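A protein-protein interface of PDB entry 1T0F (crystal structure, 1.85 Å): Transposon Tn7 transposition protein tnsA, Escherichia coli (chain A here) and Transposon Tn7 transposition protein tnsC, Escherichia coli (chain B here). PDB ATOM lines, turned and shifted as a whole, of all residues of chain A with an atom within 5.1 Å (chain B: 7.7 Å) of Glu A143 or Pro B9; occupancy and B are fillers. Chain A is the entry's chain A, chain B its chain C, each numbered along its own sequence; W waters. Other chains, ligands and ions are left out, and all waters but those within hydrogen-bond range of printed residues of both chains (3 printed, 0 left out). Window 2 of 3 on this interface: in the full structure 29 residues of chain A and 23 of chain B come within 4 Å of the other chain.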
ATOM      1  N   GLN A 141     -18.593  25.494 -27.756  1.00  0.00           N
ATOM      2  CA  GLN A 141     -19.149  25.049 -29.032  1.00  0.00           C
ATOM      3  C   GLN A 141     -20.250  24.016 -28.755  1.00  0.00           C
ATOM      4  O   GLN A 141     -20.984  23.624 -29.662  1.00  0.00           O
ATOM      5  CB  GLN A 141     -18.056  24.411 -29.902  1.00  0.00           C
ATOM      6  CG  GLN A 141     -16.807  25.264 -30.061  1.00  0.00           C
ATOM      7  CD  GLN A 141     -17.043  26.539 -30.850  1.00  0.00           C
ATOM      8  OE1 GLN A 141     -16.384  27.552 -30.614  1.00  0.00           O
ATOM      9  NE2 GLN A 141     -17.973  26.493 -31.803  1.00  0.00           N
ATOM     10  N   ASP A 142     -20.369  23.586 -27.500  1.00  0.00           N
ATOM     11  CA  ASP A 142     -21.372  22.588 -27.121  1.00  0.00           C
ATOM     12  C   ASP A 142     -22.739  23.221 -26.839  1.00  0.00           C
ATOM     13  O   ASP A 142     -22.874  24.098 -25.982  1.00  0.00           O
ATOM     14  CB  ASP A 142     -20.885  21.808 -25.898  1.00  0.00           C
ATOM     15  CG  ASP A 142     -21.795  20.651 -25.544  1.00  0.00           C
ATOM     16  OD1 ASP A 142     -21.801  19.647 -26.288  1.00  0.00           O
ATOM     17  OD2 ASP A 142     -22.513  20.750 -24.525  1.00  0.00           O
ATOM     18  N   GLU A 143     -23.760  22.767 -27.558  1.00  0.00           N
ATOM     19  CA  GLU A 143     -25.101  23.313 -27.398  1.00  0.00           C
ATOM     20  C   GLU A 143     -25.673  23.237 -25.981  1.00  0.00           C
ATOM     21  O   GLU A 143     -26.224  24.222 -25.487  1.00  0.00           O
ATOM     22  CB  GLU A 143     -26.045  22.647 -28.410  1.00  0.00           C
ATOM     23  CG  GLU A 143     -25.597  22.898 -29.851  1.00  0.00           C
ATOM     24  CD  GLU A 143     -26.346  22.059 -30.871  1.00  0.00           C
ATOM     25  OE1 GLU A 143     -26.456  20.835 -30.662  1.00  0.00           O
ATOM     26  OE2 GLU A 143     -26.810  22.621 -31.887  1.00  0.00           O
ATOM     27  N   ARG A 144     -25.542  22.095 -25.315  1.00  0.00           N
ATOM     28  CA  ARG A 144     -26.071  21.984 -23.956  1.00  0.00           C
ATOM     29  C   ARG A 144     -25.296  22.894 -22.994  1.00  0.00           C
ATOM     30  O   ARG A 144     -25.878  23.491 -22.088  1.00  0.00           O
ATOM     31  CB  ARG A 144     -26.008  20.536 -23.467  1.00  0.00           C
ATOM     32  CG  ARG A 144     -26.554  20.341 -22.054  1.00  0.00           C
ATOM     33  CD  ARG A 144     -27.959  20.930 -21.923  1.00  0.00           C
ATOM     34  NE  ARG A 144     -28.577  20.611 -20.636  1.00  0.00           N
ATOM     35  CZ  ARG A 144     -29.753  21.087 -20.236  1.00  0.00           C
ATOM     36  NH1 ARG A 144     -30.443  21.909 -21.018  1.00  0.00           N
ATOM     37  NH2 ARG A 144     -30.252  20.730 -19.058  1.00  0.00           N
ATOM     38  N   THR A 145     -23.986  23.003 -23.194  1.00  0.00           N
ATOM     39  CA  THR A 145     -23.172  23.867 -22.336  1.00  0.00           C
ATOM     40  C   THR A 145     -23.686  25.288 -22.491  1.00  0.00           C
ATOM     41  O   THR A 145     -23.853  26.003 -21.500  1.00  0.00           O
ATOM     42  CB  THR A 145     -21.685  23.811 -22.717  1.00  0.00           C
ATOM     43  OG1 THR A 145     -21.183  22.500 -22.453  1.00  0.00           O
ATOM     44  CG2 THR A 145     -20.874  24.832 -21.907  1.00  0.00           C
ATOM     45  N   LEU A 146     -23.949  25.688 -23.734  1.00  0.00           N
ATOM     46  CA  LEU A 146     -24.464  27.020 -24.026  1.00  0.00           C
ATOM     47  C   LEU A 146     -25.848  27.229 -23.405  1.00  0.00           C
ATOM     48  O   LEU A 146     -26.163  28.327 -22.942  1.00  0.00           O
ATOM     49  CB  LEU A 146     -24.534  27.257 -25.544  1.00  0.00           C
ATOM     50  CG  LEU A 146     -23.197  27.393 -26.295  1.00  0.00           C
ATOM     51  CD1 LEU A 146     -23.461  27.547 -27.789  1.00  0.00           C
ATOM     52  CD2 LEU A 146     -22.416  28.614 -25.775  1.00  0.00           C
ATOM     53  N   GLU A 147     -26.683  26.191 -23.389  1.00  0.00           N
ATOM     54  CA  GLU A 147     -28.011  26.343 -22.780  1.00  0.00           C
ATOM     55  C   GLU A 147     -27.873  26.609 -21.283  1.00  0.00           C
ATOM     56  O   GLU A 147     -28.557  27.470 -20.731  1.00  0.00           O
ATOM     57  CB  GLU A 147     -28.871  25.084 -22.962  1.00  0.00           C
ATOM     58  CG  GLU A 147     -29.267  24.758 -24.383  1.00  0.00           C
ATOM     59  CD  GLU A 147     -30.237  23.587 -24.440  1.00  0.00           C
ATOM     60  OE1 GLU A 147     -29.991  22.579 -23.751  1.00  0.00           O
ATOM     61  OE2 GLU A 147     -31.244  23.678 -25.170  1.00  0.00           O
ATOM     62  N   VAL B   6     -39.553  23.854 -25.262  1.00  0.00           N
ATOM     63  CA  VAL B   6     -38.094  23.861 -25.304  1.00  0.00           C
ATOM     64  C   VAL B   6     -37.603  24.140 -26.719  1.00  0.00           C
ATOM     65  O   VAL B   6     -37.803  23.330 -27.627  1.00  0.00           O
ATOM     66  CB  VAL B   6     -37.511  22.514 -24.829  1.00  0.00           C
ATOM     67  CG1 VAL B   6     -36.015  22.462 -25.109  1.00  0.00           C
ATOM     68  CG2 VAL B   6     -37.769  22.337 -23.339  1.00  0.00           C
ATOM     69  N   VAL B   7     -36.955  25.289 -26.893  1.00  0.00           N
ATOM     70  CA  VAL B   7     -36.435  25.701 -28.192  1.00  0.00           C
ATOM     71  C   VAL B   7     -35.298  24.799 -28.663  1.00  0.00           C
ATOM     72  O   VAL B   7     -34.305  24.627 -27.963  1.00  0.00           O
ATOM     73  CB  VAL B   7     -35.921  27.150 -28.133  1.00  0.00           C
ATOM     74  CG1 VAL B   7     -35.550  27.631 -29.523  1.00  0.00           C
ATOM     75  CG2 VAL B   7     -36.980  28.048 -27.520  1.00  0.00           C
ATOM     76  N   LYS B   8     -35.453  24.222 -29.852  1.00  0.00           N
ATOM     77  CA  LYS B   8     -34.429  23.349 -30.417  1.00  0.00           C
ATOM     78  C   LYS B   8     -33.378  24.202 -31.124  1.00  0.00           C
ATOM     79  O   LYS B   8     -33.684  25.279 -31.627  1.00  0.00           O
ATOM     80  CB  LYS B   8     -35.051  22.362 -31.409  1.00  0.00           C
ATOM     81  CG  LYS B   8     -36.017  21.367 -30.774  1.00  0.00           C
ATOM     82  CD  LYS B   8     -36.517  20.353 -31.796  1.00  0.00           C
ATOM     83  CE  LYS B   8     -37.490  19.363 -31.166  1.00  0.00           C
ATOM     84  NZ  LYS B   8     -37.990  18.360 -32.153  1.00  0.00           N
ATOM     85  N   PRO B   9     -32.126  23.726 -31.166  1.00  0.00           N
ATOM     86  CA  PRO B   9     -31.025  24.448 -31.809  1.00  0.00           C
ATOM     87  C   PRO B   9     -31.364  25.062 -33.168  1.00  0.00           C
ATOM     88  O   PRO B   9     -30.886  26.149 -33.502  1.00  0.00           O
ATOM     89  CB  PRO B   9     -29.935  23.387 -31.902  1.00  0.00           C
ATOM     90  CG  PRO B   9     -30.150  22.602 -30.652  1.00  0.00           C
ATOM     91  CD  PRO B   9     -31.655  22.437 -30.625  1.00  0.00           C
ATOM     92  N   SER B  10     -32.198  24.376 -33.945  1.00  0.00           N
ATOM     93  CA  SER B  10     -32.571  24.865 -35.268  1.00  0.00           C
ATOM     94  C   SER B  10     -33.367  26.163 -35.215  1.00  0.00           C
ATOM     95  O   SER B  10     -33.443  26.884 -36.208  1.00  0.00           O
ATOM     96  CB  SER B  10     -33.370  23.797 -36.029  1.00  0.00           C
ATOM     97  OG  SER B  10     -34.641  23.586 -35.442  1.00  0.00           O
ATOM     98  N   ASP B  11     -33.952  26.470 -34.060  1.00  0.00           N
ATOM     99  CA  ASP B  11     -34.735  27.695 -33.917  1.00  0.00           C
ATOM    100  C   ASP B  11     -34.060  28.745 -33.037  1.00  0.00           C
ATOM    101  O   ASP B  11     -34.679  29.734 -32.651  1.00  0.00           O
ATOM    102  CB  ASP B  11     -36.126  27.380 -33.352  1.00  0.00           C
ATOM    103  CG  ASP B  11     -36.990  26.594 -34.330  1.00  0.00           C
ATOM    104  OD1 ASP B  11     -37.103  27.024 -35.498  1.00  0.00           O
ATOM    105  OD2 ASP B  11     -37.558  25.554 -33.928  1.00  0.00           O
ATOM    106  N   TRP B  12     -32.789  28.542 -32.722  1.00  0.00           N
ATOM    107  CA  TRP B  12     -32.082  29.505 -31.885  1.00  0.00           C
ATOM    108  C   TRP B  12     -31.961  30.880 -32.537  1.00  0.00           C
ATOM    109  O   TRP B  12     -31.819  31.886 -31.843  1.00  0.00           O
ATOM    110  CB  TRP B  12     -30.695  28.966 -31.522  1.00  0.00           C
ATOM    111  CG  TRP B  12     -30.728  27.924 -30.430  1.00  0.00           C
ATOM    112  CD1 TRP B  12     -31.839  27.405 -29.819  1.00  0.00           C
ATOM    113  CD2 TRP B  12     -29.601  27.296 -29.810  1.00  0.00           C
ATOM    114  NE1 TRP B  12     -31.471  26.495 -28.859  1.00  0.00           N
ATOM    115  CE2 TRP B  12     -30.104  26.407 -28.830  1.00  0.00           C
ATOM    116  CE3 TRP B  12     -28.213  27.396 -29.984  1.00  0.00           C
ATOM    117  CZ2 TRP B  12     -29.269  25.625 -28.030  1.00  0.00           C
ATOM    118  CZ3 TRP B  12     -27.382  26.620 -29.188  1.00  0.00           C
ATOM    119  CH2 TRP B  12     -27.915  25.742 -28.219  1.00  0.00           C
ATOM    120  N   ASP B  13     -32.049  30.933 -33.863  1.00  0.00           N
ATOM    121  CA  ASP B  13     -31.928  32.204 -34.566  1.00  0.00           C
ATOM    122  C   ASP B  13     -33.117  33.136 -34.342  1.00  0.00           C
ATOM    123  O   ASP B  13     -33.125  34.267 -34.827  1.00  0.00           O
ATOM    124  CB  ASP B  13     -31.719  31.966 -36.072  1.00  0.00           C
ATOM    125  CG  ASP B  13     -32.949  31.396 -36.758  1.00  0.00           C
ATOM    126  OD1 ASP B  13     -33.486  30.374 -36.281  1.00  0.00           O
ATOM    127  OD2 ASP B  13     -33.371  31.972 -37.784  1.00  0.00           O
ATOM    128  N   SER B  14     -34.110  32.664 -33.592  1.00  0.00           N
ATOM    129  CA  SER B  14     -35.299  33.458 -33.292  1.00  0.00           C
ATOM    130  C   SER B  14     -35.263  34.051 -31.880  1.00  0.00           C
ATOM    131  O   SER B  14     -36.150  34.814 -31.499  1.00  0.00           O
ATOM    132  CB  SER B  14     -36.554  32.593 -33.428  1.00  0.00           C
ATOM    133  OG  SER B  14     -36.551  31.555 -32.459  1.00  0.00           O
ATOM    134  N   LEU B  15     -34.234  33.702 -31.111  1.00  0.00           N
ATOM    135  CA  LEU B  15     -34.096  34.181 -29.734  1.00  0.00           C
ATOM    136  C   LEU B  15     -33.587  35.625 -29.637  1.00  0.00           C
ATOM    137  O   LEU B  15     -33.163  36.206 -30.632  1.00  0.00           O
ATOM    138  CB  LEU B  15     -33.174  33.232 -28.965  1.00  0.00           C
ATOM    139  CG  LEU B  15     -33.707  31.799 -28.847  1.00  0.00           C
ATOM    140  CD1 LEU B  15     -32.629  30.877 -28.313  1.00  0.00           C
ATOM    141  CD2 LEU B  15     -34.931  31.783 -27.949  1.00  0.00           C
ATOM    142  N   ARG B  21     -27.623  31.564 -27.042  1.00  0.00           N
ATOM    143  CA  ARG B  21     -28.039  30.639 -28.093  1.00  0.00           C
ATOM    144  C   ARG B  21     -28.193  31.373 -29.428  1.00  0.00           C
ATOM    145  O   ARG B  21     -27.816  30.849 -30.477  1.00  0.00           O
ATOM    146  CB  ARG B  21     -29.355  29.964 -27.701  1.00  0.00           C
ATOM    147  CG  ARG B  21     -29.224  29.022 -26.514  1.00  0.00           C
ATOM    148  CD  ARG B  21     -30.589  28.541 -26.047  1.00  0.00           C
ATOM    149  NE  ARG B  21     -31.388  29.637 -25.508  1.00  0.00           N
ATOM    150  CZ  ARG B  21     -32.669  29.525 -25.162  1.00  0.00           C
ATOM    151  NH1 ARG B  21     -33.295  28.363 -25.304  1.00  0.00           N
ATOM    152  NH2 ARG B  21     -33.321  30.571 -24.671  1.00  0.00           N
ATOM    153  N   TYR B  24     -24.756  32.238 -30.792  1.00  0.00           N
ATOM    154  CA  TYR B  24     -24.145  31.068 -31.393  1.00  0.00           C
ATOM    155  C   TYR B  24     -24.691  30.840 -32.802  1.00  0.00           C
ATOM    156  O   TYR B  24     -23.930  30.551 -33.727  1.00  0.00           O
ATOM    157  CB  TYR B  24     -24.427  29.828 -30.544  1.00  0.00           C
ATOM    158  CG  TYR B  24     -23.883  28.546 -31.135  1.00  0.00           C
ATOM    159  CD1 TYR B  24     -22.521  28.255 -31.089  1.00  0.00           C
ATOM    160  CD2 TYR B  24     -24.735  27.622 -31.747  1.00  0.00           C
ATOM    161  CE1 TYR B  24     -22.016  27.069 -31.637  1.00  0.00           C
ATOM    162  CE2 TYR B  24     -24.240  26.439 -32.300  1.00  0.00           C
ATOM    163  CZ  TYR B  24     -22.883  26.170 -32.240  1.00  0.00           C
ATOM    164  OH  TYR B  24     -22.391  25.002 -32.784  1.00  0.00           O
ATOM    165  N   SER B  25     -26.005  30.980 -32.961  1.00  0.00           N
ATOM    166  CA  SER B  25     -26.639  30.745 -34.258  1.00  0.00           C
ATOM    167  C   SER B  25     -26.198  31.704 -35.359  1.00  0.00           C
ATOM    168  O   SER B  25     -26.157  31.328 -36.530  1.00  0.00           O
ATOM    169  CB  SER B  25     -28.166  30.798 -34.126  1.00  0.00           C
ATOM    170  OG  SER B  25     -28.646  32.126 -33.978  1.00  0.00           O
HETATM  171  O   HOH W   1     -32.644  25.707 -26.059  1.00  0.00           O
HETATM  172  O   HOH W   2     -21.811  22.169 -31.642  1.00  0.00           O
HETATM  173  O   HOH W   3     -19.326  24.244 -33.474  1.00  0.00           O
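OE1 of Glu A147 is in salt-bridge range of NH1 of Arg A144 (2.8 Å).
O of Gln A141 touches OH of Tyr B24 (3.7 Å).
OE2 of Glu A143 touches CB of Pro B9, at 3.2 Å.
Trp B12 touches Glu A143.
Tyr B24 touches Leu A146.
CZ2 of Trp B12 touches CG of Glu A147, at 3.7 Å.
Of the printed residues of chain B, Glu A143 touches Pro B9 and Trp B12.
Of the printed residues of chain B, Glu A147 touches Trp B12.
Val B7 touches none of the printed residues of chain A.
Asp B11 touches none of the printed residues of chain A.
Printed residues of chain A within 4 Å of Trp B12: Glu A143 (3.6 Å) and Glu A147 (3.7 Å).
Of the printed residues of chain A, Tyr B24 touches Gln A141 and Leu A146.
The nearest residue of chain B that does not touch Glu A143 is Tyr B24 (4.5 Å).
The nearest printed residue of chain A that does not touch Pro B9 is Glu A147 (5.6 Å).
Of the 13 printed residues of chain B, 3 touch a printed residue of chain A.
Printed residues of chain B that touch a printed residue of chain A: Pro B9, Trp B12 and Tyr B24.
Hydrophobic or aromatic side chains of chain B within 4 Å of the printed part of chain A: Pro B9, Trp B12 and Tyr B24.
Of the 7 printed residues of chain A, 4 touch a printed residue of chain B.
Printed residues of chain A that touch a printed residue of chain B: Gln A141, Glu A143, Leu A146 and Glu A147.
Hydrophobic or aromatic side chains of chain A within 4 Å of the printed part of chain B: Leu A146.
Among the printed residues, no Asp or Glu carboxylate lies within 4 Å of a Lys or Arg side-chain nitrogen of the other chain.
Water W2 lies within hydrogen-bond range of the backbone carbonyl oxygen (O) of Gln A141 and the side-chain hydroxyl (OH) of Tyr B24.
Water W1 lies within hydrogen-bond range of OE2 of Glu A147 (2.6 Å), O of Val B7 (2.7 Å), NH1 of Arg B21 (2.8 Å) and NE1 of Trp B12 (3.1 Å).
Water W3 lies within hydrogen-bond range of the side-chain amide nitrogen (NE2) of Gln A141 and the side-chain hydroxyl (OH) of Tyr B24.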
